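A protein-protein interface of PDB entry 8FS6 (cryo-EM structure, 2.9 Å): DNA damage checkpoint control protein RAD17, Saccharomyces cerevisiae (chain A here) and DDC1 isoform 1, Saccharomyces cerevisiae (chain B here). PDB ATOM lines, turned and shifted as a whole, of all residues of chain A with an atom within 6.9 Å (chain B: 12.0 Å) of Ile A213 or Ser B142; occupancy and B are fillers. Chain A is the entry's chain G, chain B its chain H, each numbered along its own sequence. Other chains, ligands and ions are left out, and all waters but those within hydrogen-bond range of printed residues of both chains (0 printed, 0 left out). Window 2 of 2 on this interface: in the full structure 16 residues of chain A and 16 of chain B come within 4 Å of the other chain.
Glu A161 touches none of the printed residues of chain B. Ala A162 touches just one residue of chain B: Ile B144 (3.7 Å). Printed residues of chain B within 4 Å of Ser A165: Ile B144. No residue of chain B comes within 4 Å of Leu A207. Of chain B, only Ser B142, Leu B143 and Ile B144 come within 4 Å of Pro A208. No residue of chain B comes within 4 Å of Asn A210. No residue of chain B comes within 4 Å of Ser A212. No residue of chain B comes within 4 Å of Glu A215. Ser B142 touches just these residues of chain A: Pro A208 and Ile A213. Printed residues of chain A within 4 Å of Leu B143: Pro A208 (3.3 Å). Printed residues of chain A within 4 Å of Ile B144: Ala A162 (3.7 Å), Ser A165 (3.7 Å) and Pro A208 (3.7 Å).
CB of Ala A162 touches CD1 of Ile B144, 3.7 Å away. Ser A165 touches Ile B144. O of Ser B142 touches CG of Pro A208, 3.4 Å away. Leu B143 touches Pro A208. Pro A208 touches Ile B144 (CG to N, 3.7 Å). Ser B142 touches Ile A213.
The backbone NH of Lys A159 is in hydrogen-bond range of the backbone carbonyl oxygen of Ile A213 (3.2 Å). The backbone carbonyl oxygen (O) of Glu A161 sits at hydrogen-bond distance from the side-chain hydroxyl (OG) of Ser A165 (3.3 Å). O of Ala A162 lies within hydrogen-bond range of OG of Ser A165, 2.5 Å away. N of Ser B142 lies within hydrogen-bond range of OD1 of Asp B111.
Printed residues of chain B that touch a printed residue of chain A: Ser B142, Leu B143 and Ile B144. Of the 19 printed residues of chain A, 4 touch a printed residue of chain B. Hydrophobic or aromatic side chains of chain A within 4 Å of the printed part of chain B: Ala A162, Pro A208 and Ile A213. Among the printed residues, no Asp or Glu carboxylate lies within 4 Å of a Lys or Arg side-chain nitrogen of the other chain.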
ATOM      1  N   ILE A 157      22.055  24.597   3.173  1.00  0.00           N
ATOM      2  CA  ILE A 157      22.113  23.151   3.353  1.00  0.00           C
ATOM      3  C   ILE A 157      21.085  22.529   2.418  1.00  0.00           C
ATOM      4  O   ILE A 157      19.886  22.812   2.528  1.00  0.00           O
ATOM      5  CB  ILE A 157      21.850  22.741   4.810  1.00  0.00           C
ATOM      6  CG1 ILE A 157      22.770  23.517   5.756  1.00  0.00           C
ATOM      7  CG2 ILE A 157      22.046  21.243   4.984  1.00  0.00           C
ATOM      8  CD1 ILE A 157      22.559  23.190   7.217  1.00  0.00           C
ATOM      9  N   ILE A 158      21.553  21.685   1.500  1.00  0.00           N
ATOM     10  CA  ILE A 158      20.711  21.072   0.481  1.00  0.00           C
ATOM     11  C   ILE A 158      20.899  19.563   0.540  1.00  0.00           C
ATOM     12  O   ILE A 158      22.021  19.075   0.713  1.00  0.00           O
ATOM     13  CB  ILE A 158      21.039  21.608  -0.932  1.00  0.00           C
ATOM     14  CG1 ILE A 158      20.960  23.137  -0.966  1.00  0.00           C
ATOM     15  CG2 ILE A 158      20.096  21.019  -1.970  1.00  0.00           C
ATOM     16  CD1 ILE A 158      22.309  23.824  -0.927  1.00  0.00           C
ATOM     17  N   LYS A 159      19.798  18.825   0.406  1.00  0.00           N
ATOM     18  CA  LYS A 159      19.869  17.370   0.405  1.00  0.00           C
ATOM     19  C   LYS A 159      20.628  16.873  -0.822  1.00  0.00           C
ATOM     20  O   LYS A 159      20.700  17.546  -1.855  1.00  0.00           O
ATOM     21  CB  LYS A 159      18.464  16.766   0.448  1.00  0.00           C
ATOM     22  CG  LYS A 159      17.774  16.663  -0.903  1.00  0.00           C
ATOM     23  CD  LYS A 159      16.375  16.079  -0.771  1.00  0.00           C
ATOM     24  CE  LYS A 159      16.374  14.811   0.069  1.00  0.00           C
ATOM     25  NZ  LYS A 159      17.219  13.742  -0.532  1.00  0.00           N
ATOM     26  N   GLY A 160      21.215  15.683  -0.690  1.00  0.00           N
ATOM     27  CA  GLY A 160      22.088  15.174  -1.734  1.00  0.00           C
ATOM     28  C   GLY A 160      21.362  14.819  -3.018  1.00  0.00           C
ATOM     29  O   GLY A 160      21.880  15.053  -4.114  1.00  0.00           O
ATOM     30  N   GLU A 161      20.163  14.243  -2.906  1.00  0.00           N
ATOM     31  CA  GLU A 161      19.480  13.713  -4.084  1.00  0.00           C
ATOM     32  C   GLU A 161      19.028  14.827  -5.022  1.00  0.00           C
ATOM     33  O   GLU A 161      19.216  14.738  -6.242  1.00  0.00           O
ATOM     34  CB  GLU A 161      18.289  12.856  -3.653  1.00  0.00           C
ATOM     35  CG  GLU A 161      18.677  11.558  -2.962  1.00  0.00           C
ATOM     36  CD  GLU A 161      19.198  10.511  -3.929  1.00  0.00           C
ATOM     37  OE1 GLU A 161      18.973  10.659  -5.149  1.00  0.00           O
ATOM     38  OE2 GLU A 161      19.836   9.542  -3.468  1.00  0.00           O
ATOM     39  N   ALA A 162      18.421  15.882  -4.471  1.00  0.00           N
ATOM     40  CA  ALA A 162      17.962  16.990  -5.304  1.00  0.00           C
ATOM     41  C   ALA A 162      19.131  17.692  -5.978  1.00  0.00           C
ATOM     42  O   ALA A 162      19.063  18.029  -7.168  1.00  0.00           O
ATOM     43  CB  ALA A 162      17.155  17.980  -4.464  1.00  0.00           C
ATOM     44  N   LEU A 163      20.216  17.916  -5.236  1.00  0.00           N
ATOM     45  CA  LEU A 163      21.394  18.539  -5.828  1.00  0.00           C
ATOM     46  C   LEU A 163      21.980  17.662  -6.928  1.00  0.00           C
ATOM     47  O   LEU A 163      22.334  18.162  -8.002  1.00  0.00           O
ATOM     48  CB  LEU A 163      22.433  18.824  -4.743  1.00  0.00           C
ATOM     49  CG  LEU A 163      23.619  19.712  -5.124  1.00  0.00           C
ATOM     50  CD1 LEU A 163      23.139  21.063  -5.632  1.00  0.00           C
ATOM     51  CD2 LEU A 163      24.558  19.890  -3.945  1.00  0.00           C
ATOM     52  N   SER A 165      20.425  15.478  -8.799  1.00  0.00           N
ATOM     53  CA  SER A 165      19.544  15.580  -9.958  1.00  0.00           C
ATOM     54  C   SER A 165      19.755  16.897 -10.696  1.00  0.00           C
ATOM     55  O   SER A 165      19.732  16.934 -11.933  1.00  0.00           O
ATOM     56  CB  SER A 165      18.086  15.435  -9.524  1.00  0.00           C
ATOM     57  OG  SER A 165      17.728  16.446  -8.597  1.00  0.00           O
ATOM     58  N   LEU A 207      15.557  25.223  -6.607  1.00  0.00           N
ATOM     59  CA  LEU A 207      15.368  24.256  -5.536  1.00  0.00           C
ATOM     60  C   LEU A 207      14.135  24.628  -4.713  1.00  0.00           C
ATOM     61  O   LEU A 207      13.879  25.813  -4.481  1.00  0.00           O
ATOM     62  CB  LEU A 207      16.600  24.202  -4.633  1.00  0.00           C
ATOM     63  CG  LEU A 207      17.701  23.203  -5.005  1.00  0.00           C
ATOM     64  CD1 LEU A 207      17.123  21.817  -5.246  1.00  0.00           C
ATOM     65  CD2 LEU A 207      18.489  23.679  -6.218  1.00  0.00           C
ATOM     66  N   PRO A 208      13.355  23.644  -4.271  1.00  0.00           N
ATOM     67  CA  PRO A 208      12.155  23.952  -3.487  1.00  0.00           C
ATOM     68  C   PRO A 208      12.504  24.546  -2.132  1.00  0.00           C
ATOM     69  O   PRO A 208      13.562  24.278  -1.559  1.00  0.00           O
ATOM     70  CB  PRO A 208      11.463  22.591  -3.334  1.00  0.00           C
ATOM     71  CG  PRO A 208      12.144  21.678  -4.302  1.00  0.00           C
ATOM     72  CD  PRO A 208      13.526  22.199  -4.482  1.00  0.00           C
ATOM     73  N   SER A 209      11.586  25.367  -1.621  1.00  0.00           N
ATOM     74  CA  SER A 209      11.789  26.046  -0.349  1.00  0.00           C
ATOM     75  C   SER A 209      11.438  25.181   0.854  1.00  0.00           C
ATOM     76  O   SER A 209      11.616  25.635   1.990  1.00  0.00           O
ATOM     77  CB  SER A 209      10.969  27.337  -0.305  1.00  0.00           C
ATOM     78  OG  SER A 209      11.166  28.024   0.918  1.00  0.00           O
ATOM     79  N   ASN A 210      10.943  23.965   0.638  1.00  0.00           N
ATOM     80  CA  ASN A 210      10.586  23.097   1.751  1.00  0.00           C
ATOM     81  C   ASN A 210      11.831  22.677   2.525  1.00  0.00           C
ATOM     82  O   ASN A 210      12.938  22.611   1.984  1.00  0.00           O
ATOM     83  CB  ASN A 210       9.831  21.864   1.250  1.00  0.00           C
ATOM     84  CG  ASN A 210      10.530  21.176   0.093  1.00  0.00           C
ATOM     85  OD1 ASN A 210      11.635  21.552  -0.296  1.00  0.00           O
ATOM     86  ND2 ASN A 210       9.885  20.158  -0.465  1.00  0.00           N
ATOM     87  N   ARG A 211      11.641  22.396   3.815  1.00  0.00           N
ATOM     88  CA  ARG A 211      12.753  22.017   4.677  1.00  0.00           C
ATOM     89  C   ARG A 211      13.292  20.625   4.373  1.00  0.00           C
ATOM     90  O   ARG A 211      14.371  20.280   4.866  1.00  0.00           O
ATOM     91  CB  ARG A 211      12.329  22.104   6.145  1.00  0.00           C
ATOM     92  CG  ARG A 211      12.884  23.316   6.884  1.00  0.00           C
ATOM     93  CD  ARG A 211      12.732  24.596   6.073  1.00  0.00           C
ATOM     94  NE  ARG A 211      11.338  24.895   5.765  1.00  0.00           N
ATOM     95  CZ  ARG A 211      10.936  25.934   5.045  1.00  0.00           C
ATOM     96  NH1 ARG A 211      11.799  26.797   4.536  1.00  0.00           N
ATOM     97  NH2 ARG A 211       9.635  26.108   4.828  1.00  0.00           N
ATOM     98  N   SER A 212      12.574  19.822   3.584  1.00  0.00           N
ATOM     99  CA  SER A 212      13.081  18.511   3.201  1.00  0.00           C
ATOM    100  C   SER A 212      14.186  18.602   2.156  1.00  0.00           C
ATOM    101  O   SER A 212      14.952  17.646   1.998  1.00  0.00           O
ATOM    102  CB  SER A 212      11.940  17.639   2.674  1.00  0.00           C
ATOM    103  OG  SER A 212      11.344  18.217   1.526  1.00  0.00           O
ATOM    104  N   ILE A 213      14.283  19.725   1.443  1.00  0.00           N
ATOM    105  CA  ILE A 213      15.306  19.938   0.427  1.00  0.00           C
ATOM    106  C   ILE A 213      16.216  21.106   0.793  1.00  0.00           C
ATOM    107  O   ILE A 213      17.444  20.984   0.761  1.00  0.00           O
ATOM    108  CB  ILE A 213      14.677  20.152  -0.968  1.00  0.00           C
ATOM    109  CG1 ILE A 213      13.972  18.871  -1.421  1.00  0.00           C
ATOM    110  CG2 ILE A 213      15.736  20.591  -1.971  1.00  0.00           C
ATOM    111  CD1 ILE A 213      13.781  18.759  -2.914  1.00  0.00           C
ATOM    112  N   LEU A 214      15.629  22.247   1.145  1.00  0.00           N
ATOM    113  CA  LEU A 214      16.378  23.410   1.616  1.00  0.00           C
ATOM    114  C   LEU A 214      16.200  23.480   3.129  1.00  0.00           C
ATOM    115  O   LEU A 214      15.288  24.135   3.637  1.00  0.00           O
ATOM    116  CB  LEU A 214      15.904  24.684   0.925  1.00  0.00           C
ATOM    117  CG  LEU A 214      16.820  25.906   1.023  1.00  0.00           C
ATOM    118  CD1 LEU A 214      18.250  25.542   0.653  1.00  0.00           C
ATOM    119  CD2 LEU A 214      16.306  27.033   0.140  1.00  0.00           C
ATOM    120  N   GLU A 215      17.078  22.779   3.855  1.00  0.00           N
ATOM    121  CA  GLU A 215      16.982  22.743   5.312  1.00  0.00           C
ATOM    122  C   GLU A 215      17.182  24.125   5.923  1.00  0.00           C
ATOM    123  O   GLU A 215      16.431  24.530   6.818  1.00  0.00           O
ATOM    124  CB  GLU A 215      18.003  21.756   5.886  1.00  0.00           C
ATOM    125  CG  GLU A 215      17.565  20.285   5.945  1.00  0.00           C
ATOM    126  CD  GLU A 215      17.413  19.603   4.587  1.00  0.00           C
ATOM    127  OE1 GLU A 215      17.319  18.357   4.571  1.00  0.00           O
ATOM    128  OE2 GLU A 215      17.408  20.281   3.540  1.00  0.00           O
ATOM    129  N   LYS A 216      18.182  24.864   5.451  1.00  0.00           N
ATOM    130  CA  LYS A 216      18.482  26.178   6.015  1.00  0.00           C
ATOM    131  C   LYS A 216      19.230  26.996   4.977  1.00  0.00           C
ATOM    132  O   LYS A 216      20.284  26.567   4.497  1.00  0.00           O
ATOM    133  CB  LYS A 216      19.308  26.046   7.295  1.00  0.00           C
ATOM    134  CG  LYS A 216      19.935  27.350   7.763  1.00  0.00           C
ATOM    135  CD  LYS A 216      21.124  27.099   8.676  1.00  0.00           C
ATOM    136  CE  LYS A 216      20.740  26.232   9.865  1.00  0.00           C
ATOM    137  NZ  LYS A 216      19.653  26.852  10.674  1.00  0.00           N
ATOM    138  N   VAL A 255      24.189  18.349   1.818  1.00  0.00           N
ATOM    139  CA  VAL A 255      25.309  19.100   1.264  1.00  0.00           C
ATOM    140  C   VAL A 255      25.265  20.515   1.820  1.00  0.00           C
ATOM    141  O   VAL A 255      24.216  21.168   1.787  1.00  0.00           O
ATOM    142  CB  VAL A 255      25.276  19.121  -0.276  1.00  0.00           C
ATOM    143  CG1 VAL A 255      26.524  19.795  -0.820  1.00  0.00           C
ATOM    144  CG2 VAL A 255      25.142  17.710  -0.828  1.00  0.00           C
ATOM    145  N   LYS B 107      12.325  12.325 -19.798  1.00  0.00           N
ATOM    146  CA  LYS B 107      11.974  11.974 -18.429  1.00  0.00           C
ATOM    147  C   LYS B 107      13.240  11.686 -17.632  1.00  0.00           C
ATOM    148  O   LYS B 107      13.972  10.749 -17.972  1.00  0.00           O
ATOM    149  CB  LYS B 107      11.057  10.758 -18.411  1.00  0.00           C
ATOM    150  CG  LYS B 107      10.123  10.699 -17.213  1.00  0.00           C
ATOM    151  CD  LYS B 107       9.145  11.862 -17.217  1.00  0.00           C
ATOM    152  CE  LYS B 107       8.001  11.622 -16.247  1.00  0.00           C
ATOM    153  NZ  LYS B 107       7.150  10.474 -16.664  1.00  0.00           N
ATOM    154  N   PRO B 108      13.542  12.459 -16.590  1.00  0.00           N
ATOM    155  CA  PRO B 108      14.721  12.158 -15.770  1.00  0.00           C
ATOM    156  C   PRO B 108      14.549  10.844 -15.024  1.00  0.00           C
ATOM    157  O   PRO B 108      13.444  10.478 -14.615  1.00  0.00           O
ATOM    158  CB  PRO B 108      14.799  13.346 -14.803  1.00  0.00           C
ATOM    159  CG  PRO B 108      13.960  14.418 -15.434  1.00  0.00           C
ATOM    160  CD  PRO B 108      12.868  13.691 -16.151  1.00  0.00           C
ATOM    161  N   ASP B 109      15.658  10.134 -14.847  1.00  0.00           N
ATOM    162  CA  ASP B 109      15.639   8.858 -14.147  1.00  0.00           C
ATOM    163  C   ASP B 109      15.750   9.088 -12.646  1.00  0.00           C
ATOM    164  O   ASP B 109      16.665   9.774 -12.179  1.00  0.00           O
ATOM    165  CB  ASP B 109      16.774   7.964 -14.640  1.00  0.00           C
ATOM    166  CG  ASP B 109      16.608   7.559 -16.093  1.00  0.00           C
ATOM    167  OD1 ASP B 109      15.585   7.935 -16.703  1.00  0.00           O
ATOM    168  OD2 ASP B 109      17.501   6.867 -16.625  1.00  0.00           O
ATOM    169  N   GLY B 110      14.815   8.513 -11.891  1.00  0.00           N
ATOM    170  CA  GLY B 110      14.745   8.690 -10.460  1.00  0.00           C
ATOM    171  C   GLY B 110      13.766   9.751 -10.003  1.00  0.00           C
ATOM    172  O   GLY B 110      13.471   9.828  -8.805  1.00  0.00           O
ATOM    173  N   ASP B 111      13.258  10.570 -10.922  1.00  0.00           N
ATOM    174  CA  ASP B 111      12.293  11.610 -10.601  1.00  0.00           C
ATOM    175  C   ASP B 111      11.154  11.573 -11.610  1.00  0.00           C
ATOM    176  O   ASP B 111      11.319  11.137 -12.752  1.00  0.00           O
ATOM    177  CB  ASP B 111      12.944  13.000 -10.590  1.00  0.00           C
ATOM    178  CG  ASP B 111      12.529  13.828  -9.390  1.00  0.00           C
ATOM    179  OD1 ASP B 111      11.674  13.360  -8.609  1.00  0.00           O
ATOM    180  OD2 ASP B 111      13.059  14.947  -9.226  1.00  0.00           O
ATOM    181  N   GLY B 112       9.986  12.037 -11.172  1.00  0.00           N
ATOM    182  CA  GLY B 112       8.818  12.062 -12.029  1.00  0.00           C
ATOM    183  C   GLY B 112       8.310  13.461 -12.304  1.00  0.00           C
ATOM    184  O   GLY B 112       8.182  14.274 -11.384  1.00  0.00           O
ATOM    185  N   ILE B 113       8.014  13.753 -13.568  1.00  0.00           N
ATOM    186  CA  ILE B 113       7.518  15.068 -13.961  1.00  0.00           C
ATOM    187  C   ILE B 113       6.045  15.154 -13.576  1.00  0.00           C
ATOM    188  O   ILE B 113       5.192  14.512 -14.195  1.00  0.00           O
ATOM    189  CB  ILE B 113       7.715  15.320 -15.460  1.00  0.00           C
ATOM    190  CG1 ILE B 113       9.205  15.345 -15.806  1.00  0.00           C
ATOM    191  CG2 ILE B 113       7.048  16.624 -15.875  1.00  0.00           C
ATOM    192  CD1 ILE B 113       9.488  15.599 -17.272  1.00  0.00           C
ATOM    193  N   LYS B 114       5.742  15.943 -12.544  1.00  0.00           N
ATOM    194  CA  LYS B 114       4.360  16.118 -12.119  1.00  0.00           C
ATOM    195  C   LYS B 114       3.611  17.136 -12.969  1.00  0.00           C
ATOM    196  O   LYS B 114       2.376  17.169 -12.924  1.00  0.00           O
ATOM    197  CB  LYS B 114       4.310  16.534 -10.646  1.00  0.00           C
ATOM    198  CG  LYS B 114       4.297  18.038 -10.413  1.00  0.00           C
ATOM    199  CD  LYS B 114       3.921  18.370  -8.978  1.00  0.00           C
ATOM    200  CE  LYS B 114       3.697  19.862  -8.795  1.00  0.00           C
ATOM    201  NZ  LYS B 114       2.668  20.392  -9.731  1.00  0.00           N
ATOM    202  N   SER B 115       4.323  17.951 -13.746  1.00  0.00           N
ATOM    203  CA  SER B 115       3.691  18.954 -14.595  1.00  0.00           C
ATOM    204  C   SER B 115       4.698  19.429 -15.630  1.00  0.00           C
ATOM    205  O   SER B 115       5.802  19.851 -15.273  1.00  0.00           O
ATOM    206  CB  SER B 115       3.181  20.140 -13.766  1.00  0.00           C
ATOM    207  OG  SER B 115       2.592  21.126 -14.596  1.00  0.00           O
ATOM    208  N   PHE B 116       4.315  19.359 -16.903  1.00  0.00           N
ATOM    209  CA  PHE B 116       5.124  19.868 -18.006  1.00  0.00           C
ATOM    210  C   PHE B 116       4.344  20.994 -18.672  1.00  0.00           C
ATOM    211  O   PHE B 116       3.387  20.740 -19.411  1.00  0.00           O
ATOM    212  CB  PHE B 116       5.458  18.761 -19.005  1.00  0.00           C
ATOM    213  CG  PHE B 116       6.362  19.203 -20.123  1.00  0.00           C
ATOM    214  CD1 PHE B 116       7.737  19.207 -19.959  1.00  0.00           C
ATOM    215  CD2 PHE B 116       5.836  19.609 -21.339  1.00  0.00           C
ATOM    216  CE1 PHE B 116       8.571  19.612 -20.985  1.00  0.00           C
ATOM    217  CE2 PHE B 116       6.664  20.016 -22.368  1.00  0.00           C
ATOM    218  CZ  PHE B 116       8.034  20.016 -22.190  1.00  0.00           C
ATOM    219  N   ILE B 138       8.951  22.977 -15.894  1.00  0.00           N
ATOM    220  CA  ILE B 138       8.809  21.579 -15.503  1.00  0.00           C
ATOM    221  C   ILE B 138       8.827  21.499 -13.984  1.00  0.00           C
ATOM    222  O   ILE B 138       9.750  22.011 -13.341  1.00  0.00           O
ATOM    223  CB  ILE B 138       9.921  20.703 -16.105  1.00  0.00           C
ATOM    224  CG1 ILE B 138       9.996  20.894 -17.620  1.00  0.00           C
ATOM    225  CG2 ILE B 138       9.693  19.240 -15.761  1.00  0.00           C
ATOM    226  CD1 ILE B 138      11.141  20.154 -18.261  1.00  0.00           C
ATOM    227  N   GLU B 139       7.810  20.857 -13.417  1.00  0.00           N
ATOM    228  CA  GLU B 139       7.728  20.607 -11.984  1.00  0.00           C
ATOM    229  C   GLU B 139       7.881  19.112 -11.748  1.00  0.00           C
ATOM    230  O   GLU B 139       7.094  18.314 -12.268  1.00  0.00           O
ATOM    231  CB  GLU B 139       6.404  21.113 -11.412  1.00  0.00           C
ATOM    232  CG  GLU B 139       6.516  22.417 -10.640  1.00  0.00           C
ATOM    233  CD  GLU B 139       6.628  22.199  -9.144  1.00  0.00           C
ATOM    234  OE1 GLU B 139       6.790  21.036  -8.722  1.00  0.00           O
ATOM    235  OE2 GLU B 139       6.549  23.192  -8.390  1.00  0.00           O
ATOM    236  N   MET B 140       8.889  18.737 -10.969  1.00  0.00           N
ATOM    237  CA  MET B 140       9.158  17.337 -10.686  1.00  0.00           C
ATOM    238  C   MET B 140       8.393  16.881  -9.446  1.00  0.00           C
ATOM    239  O   MET B 140       7.822  17.683  -8.702  1.00  0.00           O
ATOM    240  CB  MET B 140      10.658  17.106 -10.505  1.00  0.00           C
ATOM    241  CG  MET B 140      11.533  17.960 -11.407  1.00  0.00           C
ATOM    242  SD  MET B 140      11.539  17.398 -13.121  1.00  0.00           S
ATOM    243  CE  MET B 140      11.574  15.621 -12.899  1.00  0.00           C
ATOM    244  N   ASP B 141       8.384  15.563  -9.231  1.00  0.00           N
ATOM    245  CA  ASP B 141       7.767  15.014  -8.028  1.00  0.00           C
ATOM    246  C   ASP B 141       8.515  15.441  -6.774  1.00  0.00           C
ATOM    247  O   ASP B 141       7.933  15.477  -5.684  1.00  0.00           O
ATOM    248  CB  ASP B 141       7.701  13.490  -8.117  1.00  0.00           C
ATOM    249  CG  ASP B 141       6.513  13.005  -8.924  1.00  0.00           C
ATOM    250  OD1 ASP B 141       5.478  13.703  -8.938  1.00  0.00           O
ATOM    251  OD2 ASP B 141       6.612  11.924  -9.541  1.00  0.00           O
ATOM    252  N   SER B 142       9.799  15.768  -6.907  1.00  0.00           N
ATOM    253  CA  SER B 142      10.595  16.307  -5.813  1.00  0.00           C
ATOM    254  C   SER B 142      10.398  17.807  -5.629  1.00  0.00           C
ATOM    255  O   SER B 142      11.215  18.445  -4.956  1.00  0.00           O
ATOM    256  CB  SER B 142      12.076  15.998  -6.045  1.00  0.00           C
ATOM    257  OG  SER B 142      12.863  16.401  -4.939  1.00  0.00           O
ATOM    258  N   LEU B 143       9.348  18.374  -6.231  1.00  0.00           N
ATOM    259  CA  LEU B 143       8.963  19.782  -6.153  1.00  0.00           C
ATOM    260  C   LEU B 143       9.988  20.719  -6.777  1.00  0.00           C
ATOM    261  O   LEU B 143       9.870  21.942  -6.625  1.00  0.00           O
ATOM    262  CB  LEU B 143       8.684  20.225  -4.710  1.00  0.00           C
ATOM    263  CG  LEU B 143       7.241  20.150  -4.196  1.00  0.00           C
ATOM    264  CD1 LEU B 143       6.419  21.312  -4.735  1.00  0.00           C
ATOM    265  CD2 LEU B 143       6.583  18.818  -4.534  1.00  0.00           C
ATOM    266  N   ILE B 144      10.989  20.192  -7.482  1.00  0.00           N
ATOM    267  CA  ILE B 144      11.995  21.040  -8.107  1.00  0.00           C
ATOM    268  C   ILE B 144      11.412  21.671  -9.363  1.00  0.00           C
ATOM    269  O   ILE B 144      10.851  20.980 -10.224  1.00  0.00           O
ATOM    270  CB  ILE B 144      13.261  20.231  -8.427  1.00  0.00           C
ATOM    271  CG1 ILE B 144      13.735  19.469  -7.188  1.00  0.00           C
ATOM    272  CG2 ILE B 144      14.361  21.145  -8.945  1.00  0.00           C
ATOM    273  CD1 ILE B 144      14.985  18.650  -7.419  1.00  0.00           C
ATOM    274  N   VAL B 145      11.540  22.989  -9.474  1.00  0.00           N
ATOM    275  CA  VAL B 145      11.030  23.738 -10.615  1.00  0.00           C
ATOM    276  C   VAL B 145      12.198  23.997 -11.557  1.00  0.00           C
ATOM    277  O   VAL B 145      13.145  24.710 -11.207  1.00  0.00           O
ATOM    278  CB  VAL B 145      10.362  25.048 -10.180  1.00  0.00           C
ATOM    279  CG1 VAL B 145       9.677  25.713 -11.364  1.00  0.00           C
ATOM    280  CG2 VAL B 145       9.370  24.791  -9.057  1.00  0.00           C
ATOM    281  N   LYS B 146      12.133  23.421 -12.753  1.00  0.00           N
ATOM    282  CA  LYS B 146      13.156  23.599 -13.777  1.00  0.00           C
ATOM    283  C   LYS B 146      12.529  24.346 -14.948  1.00  0.00           C
ATOM    284  O   LYS B 146      11.683  23.796 -15.662  1.00  0.00           O
ATOM    285  CB  LYS B 146      13.727  22.254 -14.222  1.00  0.00           C
ATOM    286  CG  LYS B 146      14.048  21.305 -13.078  1.00  0.00           C
ATOM    287  CD  LYS B 146      14.769  20.057 -13.567  1.00  0.00           C
ATOM    288  CE  LYS B 146      14.124  19.487 -14.821  1.00  0.00           C
ATOM    289  NZ  LYS B 146      14.864  18.302 -15.337  1.00  0.00           N
